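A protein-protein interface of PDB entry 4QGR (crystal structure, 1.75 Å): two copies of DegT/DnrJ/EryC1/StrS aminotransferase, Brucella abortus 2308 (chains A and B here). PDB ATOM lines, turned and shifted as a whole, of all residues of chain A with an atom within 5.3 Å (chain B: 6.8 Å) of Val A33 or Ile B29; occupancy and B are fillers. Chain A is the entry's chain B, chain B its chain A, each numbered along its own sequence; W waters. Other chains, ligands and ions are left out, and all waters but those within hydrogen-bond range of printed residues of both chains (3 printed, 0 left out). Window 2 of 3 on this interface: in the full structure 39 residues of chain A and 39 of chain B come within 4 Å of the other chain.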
ATOM      1  N   ILE A  29      -1.296 -14.777 -15.764  1.00  0.00           N
ATOM      2  CA  ILE A  29      -2.408 -14.013 -16.293  1.00  0.00           C
ATOM      3  C   ILE A  29      -3.562 -13.914 -15.267  1.00  0.00           C
ATOM      4  O   ILE A  29      -4.103 -12.834 -15.056  1.00  0.00           O
ATOM      5  CB  ILE A  29      -2.887 -14.600 -17.623  1.00  0.00           C
ATOM      6  CG1 ILE A  29      -1.815 -14.396 -18.686  1.00  0.00           C
ATOM      7  CG2 ILE A  29      -4.201 -13.955 -18.046  1.00  0.00           C
ATOM      8  CD1 ILE A  29      -1.957 -15.299 -19.896  1.00  0.00           C
ATOM      9  N   SER A  30      -3.934 -15.016 -14.636  1.00  0.00           N
ATOM     10  CA  SER A  30      -4.975 -15.056 -13.619  1.00  0.00           C
ATOM     11  C   SER A  30      -4.708 -14.041 -12.506  1.00  0.00           C
ATOM     12  O   SER A  30      -5.601 -13.343 -12.030  1.00  0.00           O
ATOM     13  CB  SER A  30      -5.045 -16.459 -13.001  1.00  0.00           C
ATOM     14  OG  SER A  30      -5.974 -16.450 -11.956  1.00  0.00           O
ATOM     15  N   LYS A  31      -3.452 -13.991 -12.091  1.00  0.00           N
ATOM     16  CA  LYS A  31      -3.037 -13.115 -10.988  1.00  0.00           C
ATOM     17  C   LYS A  31      -3.313 -11.641 -11.334  1.00  0.00           C
ATOM     18  O   LYS A  31      -3.931 -10.885 -10.564  1.00  0.00           O
ATOM     19  CB  LYS A  31      -1.554 -13.393 -10.714  1.00  0.00           C
ATOM     20  CG  LYS A  31      -0.850 -12.453  -9.767  1.00  0.00           C
ATOM     21  CD  LYS A  31       0.387 -13.160  -9.223  1.00  0.00           C
ATOM     22  CE  LYS A  31       1.305 -12.185  -8.522  1.00  0.00           C
ATOM     23  NZ  LYS A  31       1.010 -12.161  -7.078  1.00  0.00           N
ATOM     24  N   VAL A  32      -2.898 -11.253 -12.530  1.00  0.00           N
ATOM     25  CA  VAL A  32      -3.151  -9.889 -13.005  1.00  0.00           C
ATOM     26  C   VAL A  32      -4.642  -9.595 -13.097  1.00  0.00           C
ATOM     27  O   VAL A  32      -5.113  -8.568 -12.616  1.00  0.00           O
ATOM     28  CB  VAL A  32      -2.504  -9.636 -14.353  1.00  0.00           C
ATOM     29  CG1 VAL A  32      -2.933  -8.286 -14.938  1.00  0.00           C
ATOM     30  CG2 VAL A  32      -1.006  -9.686 -14.229  1.00  0.00           C
ATOM     31  N   VAL A  33      -5.399 -10.504 -13.705  1.00  0.00           N
ATOM     32  CA  VAL A  33      -6.832 -10.284 -13.853  1.00  0.00           C
ATOM     33  C   VAL A  33      -7.503  -9.982 -12.508  1.00  0.00           C
ATOM     34  O   VAL A  33      -8.281  -9.016 -12.393  1.00  0.00           O
ATOM     35  CB  VAL A  33      -7.508 -11.463 -14.588  1.00  0.00           C
ATOM     36  CG1 VAL A  33      -9.025 -11.383 -14.496  1.00  0.00           C
ATOM     37  CG2 VAL A  33      -7.034 -11.497 -16.013  1.00  0.00           C
ATOM     38  N   ALA A  34      -7.176 -10.767 -11.488  1.00  0.00           N
ATOM     39  CA  ALA A  34      -7.805 -10.662 -10.194  1.00  0.00           C
ATOM     40  C   ALA A  34      -7.338  -9.421  -9.430  1.00  0.00           C
ATOM     41  O   ALA A  34      -8.112  -8.880  -8.644  1.00  0.00           O
ATOM     42  CB  ALA A  34      -7.519 -11.913  -9.355  1.00  0.00           C
ATOM     43  N   GLU A  35      -6.090  -9.007  -9.625  1.00  0.00           N
ATOM     44  CA  GLU A  35      -5.542  -7.928  -8.783  1.00  0.00           C
ATOM     45  C   GLU A  35      -6.075  -6.555  -9.179  1.00  0.00           C
ATOM     46  O   GLU A  35      -6.189  -5.635  -8.342  1.00  0.00           O
ATOM     47  CB  GLU A  35      -4.009  -7.909  -8.812  1.00  0.00           C
ATOM     48  CG  GLU A  35      -3.449  -7.021  -7.695  1.00  0.00           C
ATOM     49  CD  GLU A  35      -1.953  -7.037  -7.535  1.00  0.00           C
ATOM     50  OE1 GLU A  35      -1.213  -7.672  -8.318  1.00  0.00           O
ATOM     51  OE2 GLU A  35      -1.498  -6.454  -6.548  1.00  0.00           O
ATOM     52  N   GLY A  36      -6.384  -6.405 -10.473  1.00  0.00           N
ATOM     53  CA  GLY A  36      -6.997  -5.180 -10.955  1.00  0.00           C
ATOM     54  C   GLY A  36      -6.070  -3.980 -11.063  1.00  0.00           C
ATOM     55  O   GLY A  36      -6.558  -2.875 -10.994  1.00  0.00           O
ATOM     56  N   TYR A  38      -4.216  -2.871 -13.727  1.00  0.00           N
ATOM     57  CA  TYR A  38      -4.034  -3.168 -15.157  1.00  0.00           C
ATOM     58  C   TYR A  38      -3.110  -2.219 -15.881  1.00  0.00           C
ATOM     59  O   TYR A  38      -2.613  -2.564 -16.967  1.00  0.00           O
ATOM     60  CB  TYR A  38      -5.401  -3.219 -15.907  1.00  0.00           C
ATOM     61  CG  TYR A  38      -6.419  -4.147 -15.261  1.00  0.00           C
ATOM     62  CD1 TYR A  38      -6.148  -5.481 -15.074  1.00  0.00           C
ATOM     63  CD2 TYR A  38      -7.635  -3.673 -14.820  1.00  0.00           C
ATOM     64  CE1 TYR A  38      -7.058  -6.311 -14.462  1.00  0.00           C
ATOM     65  CE2 TYR A  38      -8.561  -4.523 -14.201  1.00  0.00           C
ATOM     66  CZ  TYR A  38      -8.243  -5.850 -14.029  1.00  0.00           C
ATOM     67  OH  TYR A  38      -9.121  -6.734 -13.443  1.00  0.00           O
ATOM     68  N   ILE A 248      -0.788  -6.994 -17.835  1.00  0.00           N
ATOM     69  CA  ILE A 248      -1.045  -8.352 -18.317  1.00  0.00           C
ATOM     70  C   ILE A 248       0.065  -8.864 -19.223  1.00  0.00           C
ATOM     71  O   ILE A 248       0.453 -10.039 -19.170  1.00  0.00           O
ATOM     72  CB  ILE A 248      -2.423  -8.484 -18.967  1.00  0.00           C
ATOM     73  CG1 ILE A 248      -2.850  -9.965 -19.090  1.00  0.00           C
ATOM     74  CG2 ILE A 248      -2.465  -7.770 -20.306  1.00  0.00           C
ATOM     75  CD1 ILE A 248      -4.356 -10.138 -19.204  1.00  0.00           C
ATOM     76  N   ARG B  18     -16.198  -6.768 -12.476  1.00  0.00           N
ATOM     77  CA  ARG B  18     -15.624  -8.026 -12.871  1.00  0.00           C
ATOM     78  C   ARG B  18     -16.418  -9.169 -12.233  1.00  0.00           C
ATOM     79  O   ARG B  18     -16.630 -10.213 -12.877  1.00  0.00           O
ATOM     80  CB  ARG B  18     -14.143  -8.087 -12.509  1.00  0.00           C
ATOM     81  CG  ARG B  18     -13.441  -9.329 -13.024  1.00  0.00           C
ATOM     82  CD  ARG B  18     -11.944  -9.311 -12.756  1.00  0.00           C
ATOM     83  NE  ARG B  18     -11.655  -9.715 -11.396  1.00  0.00           N
ATOM     84  CZ  ARG B  18     -11.682 -10.991 -10.949  1.00  0.00           C
ATOM     85  NH1 ARG B  18     -11.942 -12.042 -11.740  1.00  0.00           N
ATOM     86  NH2 ARG B  18     -11.425 -11.241  -9.674  1.00  0.00           N
ATOM     87  N   GLU B  22     -17.574 -12.408 -14.167  1.00  0.00           N
ATOM     88  CA  GLU B  22     -16.286 -13.016 -13.882  1.00  0.00           C
ATOM     89  C   GLU B  22     -15.914 -14.178 -14.797  1.00  0.00           C
ATOM     90  O   GLU B  22     -14.823 -14.233 -15.408  1.00  0.00           O
ATOM     91  CB  GLU B  22     -16.276 -13.433 -12.383  1.00  0.00           C
ATOM     92  CG  GLU B  22     -15.011 -14.172 -11.982  1.00  0.00           C
ATOM     93  CD  GLU B  22     -14.959 -14.643 -10.532  1.00  0.00           C
ATOM     94  OE1 GLU B  22     -15.747 -14.197  -9.694  1.00  0.00           O
ATOM     95  OE2 GLU B  22     -14.091 -15.488 -10.238  1.00  0.00           O
ATOM     96  N   ARG B  24     -17.394 -15.147 -17.606  1.00  0.00           N
ATOM     97  CA  ARG B  24     -17.413 -14.743 -19.020  1.00  0.00           C
ATOM     98  C   ARG B  24     -16.090 -14.057 -19.394  1.00  0.00           C
ATOM     99  O   ARG B  24     -15.504 -14.342 -20.442  1.00  0.00           O
ATOM    100  CB  ARG B  24     -18.588 -13.820 -19.317  1.00  0.00           C
ATOM    101  CG  ARG B  24     -19.993 -14.457 -19.150  1.00  0.00           C
ATOM    102  CD  ARG B  24     -21.054 -13.600 -19.829  1.00  0.00           C
ATOM    103  NE  ARG B  24     -20.928 -13.740 -21.281  1.00  0.00           N
ATOM    104  CZ  ARG B  24     -21.367 -14.775 -21.998  1.00  0.00           C
ATOM    105  NH1 ARG B  24     -22.085 -15.764 -21.469  1.00  0.00           N
ATOM    106  NH2 ARG B  24     -21.140 -14.806 -23.297  1.00  0.00           N
ATOM    107  N   LEU B  25     -15.582 -13.226 -18.501  1.00  0.00           N
ATOM    108  CA  LEU B  25     -14.285 -12.579 -18.787  1.00  0.00           C
ATOM    109  C   LEU B  25     -13.184 -13.638 -18.842  1.00  0.00           C
ATOM    110  O   LEU B  25     -12.339 -13.604 -19.755  1.00  0.00           O
ATOM    111  CB  LEU B  25     -13.970 -11.512 -17.749  1.00  0.00           C
ATOM    112  CG  LEU B  25     -14.797 -10.241 -17.910  1.00  0.00           C
ATOM    113  CD1 LEU B  25     -14.773  -9.392 -16.648  1.00  0.00           C
ATOM    114  CD2 LEU B  25     -14.275  -9.448 -19.098  1.00  0.00           C
ATOM    115  N   ASN B  26     -13.179 -14.575 -17.875  1.00  0.00           N
ATOM    116  CA  ASN B  26     -12.158 -15.628 -17.888  1.00  0.00           C
ATOM    117  C   ASN B  26     -12.167 -16.422 -19.185  1.00  0.00           C
ATOM    118  O   ASN B  26     -11.109 -16.697 -19.754  1.00  0.00           O
ATOM    119  CB  ASN B  26     -12.238 -16.558 -16.688  1.00  0.00           C
ATOM    120  CG  ASN B  26     -11.899 -15.861 -15.403  1.00  0.00           C
ATOM    121  OD1 ASN B  26     -11.233 -14.829 -15.399  1.00  0.00           O
ATOM    122  ND2 ASN B  26     -12.368 -16.399 -14.313  1.00  0.00           N
ATOM    123  N   ALA B  27     -13.357 -16.804 -19.637  1.00  0.00           N
ATOM    124  CA  ALA B  27     -13.479 -17.590 -20.871  1.00  0.00           C
ATOM    125  C   ALA B  27     -13.017 -16.810 -22.085  1.00  0.00           C
ATOM    126  O   ALA B  27     -12.366 -17.373 -22.979  1.00  0.00           O
ATOM    127  CB  ALA B  27     -14.891 -18.078 -21.083  1.00  0.00           C
ATOM    128  N   ALA B  28     -13.363 -15.527 -22.125  1.00  0.00           N
ATOM    129  CA  ALA B  28     -13.015 -14.677 -23.301  1.00  0.00           C
ATOM    130  C   ALA B  28     -11.500 -14.557 -23.398  1.00  0.00           C
ATOM    131  O   ALA B  28     -10.934 -14.681 -24.473  1.00  0.00           O
ATOM    132  CB  ALA B  28     -13.687 -13.315 -23.185  1.00  0.00           C
ATOM    133  N   ILE B  29     -10.856 -14.368 -22.243  1.00  0.00           N
ATOM    134  CA  ILE B  29      -9.415 -14.236 -22.162  1.00  0.00           C
ATOM    135  C   ILE B  29      -8.767 -15.579 -22.495  1.00  0.00           C
ATOM    136  O   ILE B  29      -7.836 -15.643 -23.283  1.00  0.00           O
ATOM    137  CB  ILE B  29      -8.997 -13.717 -20.751  1.00  0.00           C
ATOM    138  CG1 ILE B  29      -9.385 -12.240 -20.602  1.00  0.00           C
ATOM    139  CG2 ILE B  29      -7.509 -13.845 -20.575  1.00  0.00           C
ATOM    140  CD1 ILE B  29      -9.274 -11.745 -19.176  1.00  0.00           C
ATOM    141  N   SER B  30      -9.273 -16.672 -21.927  1.00  0.00           N
ATOM    142  CA  SER B  30      -8.699 -17.982 -22.185  1.00  0.00           C
ATOM    143  C   SER B  30      -8.782 -18.370 -23.655  1.00  0.00           C
ATOM    144  O   SER B  30      -7.872 -19.015 -24.179  1.00  0.00           O
ATOM    145  CB  SER B  30      -9.363 -19.029 -21.301  1.00  0.00           C
ATOM    146  OG  SER B  30      -9.008 -18.744 -19.972  1.00  0.00           O
ATOM    147  N   LYS B  31      -9.871 -17.984 -24.317  1.00  0.00           N
ATOM    148  CA  LYS B  31     -10.057 -18.293 -25.738  1.00  0.00           C
ATOM    149  C   LYS B  31      -8.975 -17.611 -26.562  1.00  0.00           C
ATOM    150  O   LYS B  31      -8.394 -18.218 -27.460  1.00  0.00           O
ATOM    151  CB  LYS B  31     -11.438 -17.837 -26.225  1.00  0.00           C
ATOM    152  CG  LYS B  31     -11.703 -18.036 -27.715  1.00  0.00           C
ATOM    153  CD  LYS B  31     -13.049 -17.420 -28.151  1.00  0.00           C
ATOM    154  CE  LYS B  31     -13.275 -17.506 -29.675  1.00  0.00           C
ATOM    155  NZ  LYS B  31     -12.418 -16.590 -30.520  1.00  0.00           N
ATOM    156  N   VAL B  32      -8.701 -16.334 -26.267  1.00  0.00           N
ATOM    157  CA  VAL B  32      -7.665 -15.611 -26.989  1.00  0.00           C
ATOM    158  C   VAL B  32      -6.290 -16.234 -26.738  1.00  0.00           C
ATOM    159  O   VAL B  32      -5.483 -16.448 -27.670  1.00  0.00           O
ATOM    160  CB  VAL B  32      -7.664 -14.111 -26.619  1.00  0.00           C
ATOM    161  CG1 VAL B  32      -6.416 -13.415 -27.108  1.00  0.00           C
ATOM    162  CG2 VAL B  32      -8.917 -13.426 -27.177  1.00  0.00           C
ATOM    163  N   VAL B  33      -5.991 -16.475 -25.473  1.00  0.00           N
ATOM    164  CA  VAL B  33      -4.719 -17.092 -25.099  1.00  0.00           C
ATOM    165  C   VAL B  33      -4.479 -18.392 -25.909  1.00  0.00           C
ATOM    166  O   VAL B  33      -3.387 -18.572 -26.504  1.00  0.00           O
ATOM    167  CB  VAL B  33      -4.623 -17.329 -23.583  1.00  0.00           C
ATOM    168  CG1 VAL B  33      -3.426 -18.233 -23.246  1.00  0.00           C
ATOM    169  CG2 VAL B  33      -4.507 -15.986 -22.857  1.00  0.00           C
ATOM    170  N   ALA B  34      -5.499 -19.244 -25.980  1.00  0.00           N
ATOM    171  CA  ALA B  34      -5.403 -20.552 -26.631  1.00  0.00           C
ATOM    172  C   ALA B  34      -5.263 -20.453 -28.151  1.00  0.00           C
ATOM    173  O   ALA B  34      -4.526 -21.232 -28.762  1.00  0.00           O
ATOM    174  CB  ALA B  34      -6.612 -21.410 -26.274  1.00  0.00           C
ATOM    175  N   TYR B 204      -8.721  -3.975 -19.888  1.00  0.00           N
ATOM    176  CA  TYR B 204      -7.793  -4.355 -18.822  1.00  0.00           C
ATOM    177  C   TYR B 204      -6.344  -4.104 -19.264  1.00  0.00           C
ATOM    178  O   TYR B 204      -5.488  -4.928 -19.093  1.00  0.00           O
ATOM    179  CB  TYR B 204      -8.040  -5.822 -18.430  1.00  0.00           C
ATOM    180  CG  TYR B 204      -9.323  -6.125 -17.651  1.00  0.00           C
ATOM    181  CD1 TYR B 204     -10.092  -5.117 -17.085  1.00  0.00           C
ATOM    182  CD2 TYR B 204      -9.740  -7.443 -17.444  1.00  0.00           C
ATOM    183  CE1 TYR B 204     -11.221  -5.399 -16.344  1.00  0.00           C
ATOM    184  CE2 TYR B 204     -10.867  -7.736 -16.694  1.00  0.00           C
ATOM    185  CZ  TYR B 204     -11.615  -6.718 -16.169  1.00  0.00           C
ATOM    186  OH  TYR B 204     -12.713  -7.007 -15.380  1.00  0.00           O
ATOM    187  N   ILE B 248      -6.663  -9.686 -27.084  1.00  0.00           N
ATOM    188  CA  ILE B 248      -7.039  -9.998 -25.703  1.00  0.00           C
ATOM    189  C   ILE B 248      -7.861  -8.876 -25.080  1.00  0.00           C
ATOM    190  O   ILE B 248      -8.806  -9.146 -24.324  1.00  0.00           O
ATOM    191  CB  ILE B 248      -5.776 -10.366 -24.889  1.00  0.00           C
ATOM    192  CG1 ILE B 248      -6.147 -11.152 -23.651  1.00  0.00           C
ATOM    193  CG2 ILE B 248      -4.921  -9.149 -24.561  1.00  0.00           C
ATOM    194  CD1 ILE B 248      -4.965 -11.722 -22.919  1.00  0.00           C
ATOM    195  N   ALA B 251     -11.448  -8.870 -26.537  1.00  0.00           N
ATOM    196  CA  ALA B 251     -12.231  -9.964 -25.952  1.00  0.00           C
ATOM    197  C   ALA B 251     -12.831  -9.508 -24.625  1.00  0.00           C
ATOM    198  O   ALA B 251     -14.029  -9.741 -24.348  1.00  0.00           O
ATOM    199  CB  ALA B 251     -11.347 -11.150 -25.763  1.00  0.00           C
ATOM    200  N   VAL B 252     -12.026  -8.821 -23.813  1.00  0.00           N
ATOM    201  CA  VAL B 252     -12.548  -8.163 -22.606  1.00  0.00           C
ATOM    202  C   VAL B 252     -13.696  -7.190 -22.928  1.00  0.00           C
ATOM    203  O   VAL B 252     -14.791  -7.221 -22.310  1.00  0.00           O
ATOM    204  CB  VAL B 252     -11.393  -7.479 -21.823  1.00  0.00           C
ATOM    205  CG1 VAL B 252     -11.945  -6.582 -20.725  1.00  0.00           C
ATOM    206  CG2 VAL B 252     -10.503  -8.545 -21.222  1.00  0.00           C
HETATM  207  O   HOH W   1      -2.957  -5.042 -17.987  1.00  0.00           O
HETATM  208  O   HOH W   2     -11.017  -7.843  -9.467  1.00  0.00           O
HETATM  209  O   HOH W   3     -10.065 -10.219  -7.246  1.00  0.00           O
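OH of Tyr A38 is in hydrogen-bond range of O of Val A33 (2.6 Å).
Among the printed residues, pairs that only touch across the chains: Tyr A38 with Tyr B204 (3.3 Å), Val A33 with Arg B18 (3.6 Å), Ala A34 with Arg B18 (3.7 Å), Tyr A38 with Arg B18 (3.9 Å), Val A33 with Ile B29 (3.9 Å) and Ile A29 with Val B33 (3.97 Å).
Printed residues of chain B within 4 Å of Ile A29: Val B33.
Of chain B, only Arg B18 and Ile B29 come within 4 Å of Val A33.
Printed residues of chain B within 4 Å of Ala A34: Arg B18.
Of chain A, only Val A33 comes within 4 Å of Ile B29.
The nearest residue of chain B that does not touch Val A33 is Asn B26 (4.2 Å).
Hydrophobic or aromatic side chains of chain B within 4 Å of the printed part of chain A: Ile B29, Val B33 and Tyr B204.
Hydrophobic or aromatic side chains of chain A within 4 Å of the printed part of chain B: Ile A29, Val A33, Ala A34 and Tyr A38.
Along chain A the printed residues that touch a printed residue of chain B span positions 29 to 38.
Among the printed residues, no Asp or Glu carboxylate lies within 4 Å of a Lys or Arg side-chain nitrogen of the other chain.
Ile A29 touches Val B33, and with the chains exchanged Val A33 touches Ile B29.
Positions printed for both chains: 29, 30, 31, 32, 33, 34 and 248.
Water W1 lies within hydrogen-bond range of O of Tyr A38, O of Tyr B204 and N of Ile A248.
Water W3 bridges O of Ala A34 (2.7 Å) and NH2 of Arg B18 (3.0 Å).
Water W2 bridges NE of Arg B18 (2.8 Å) and O of Ala A34 (3.2 Å).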
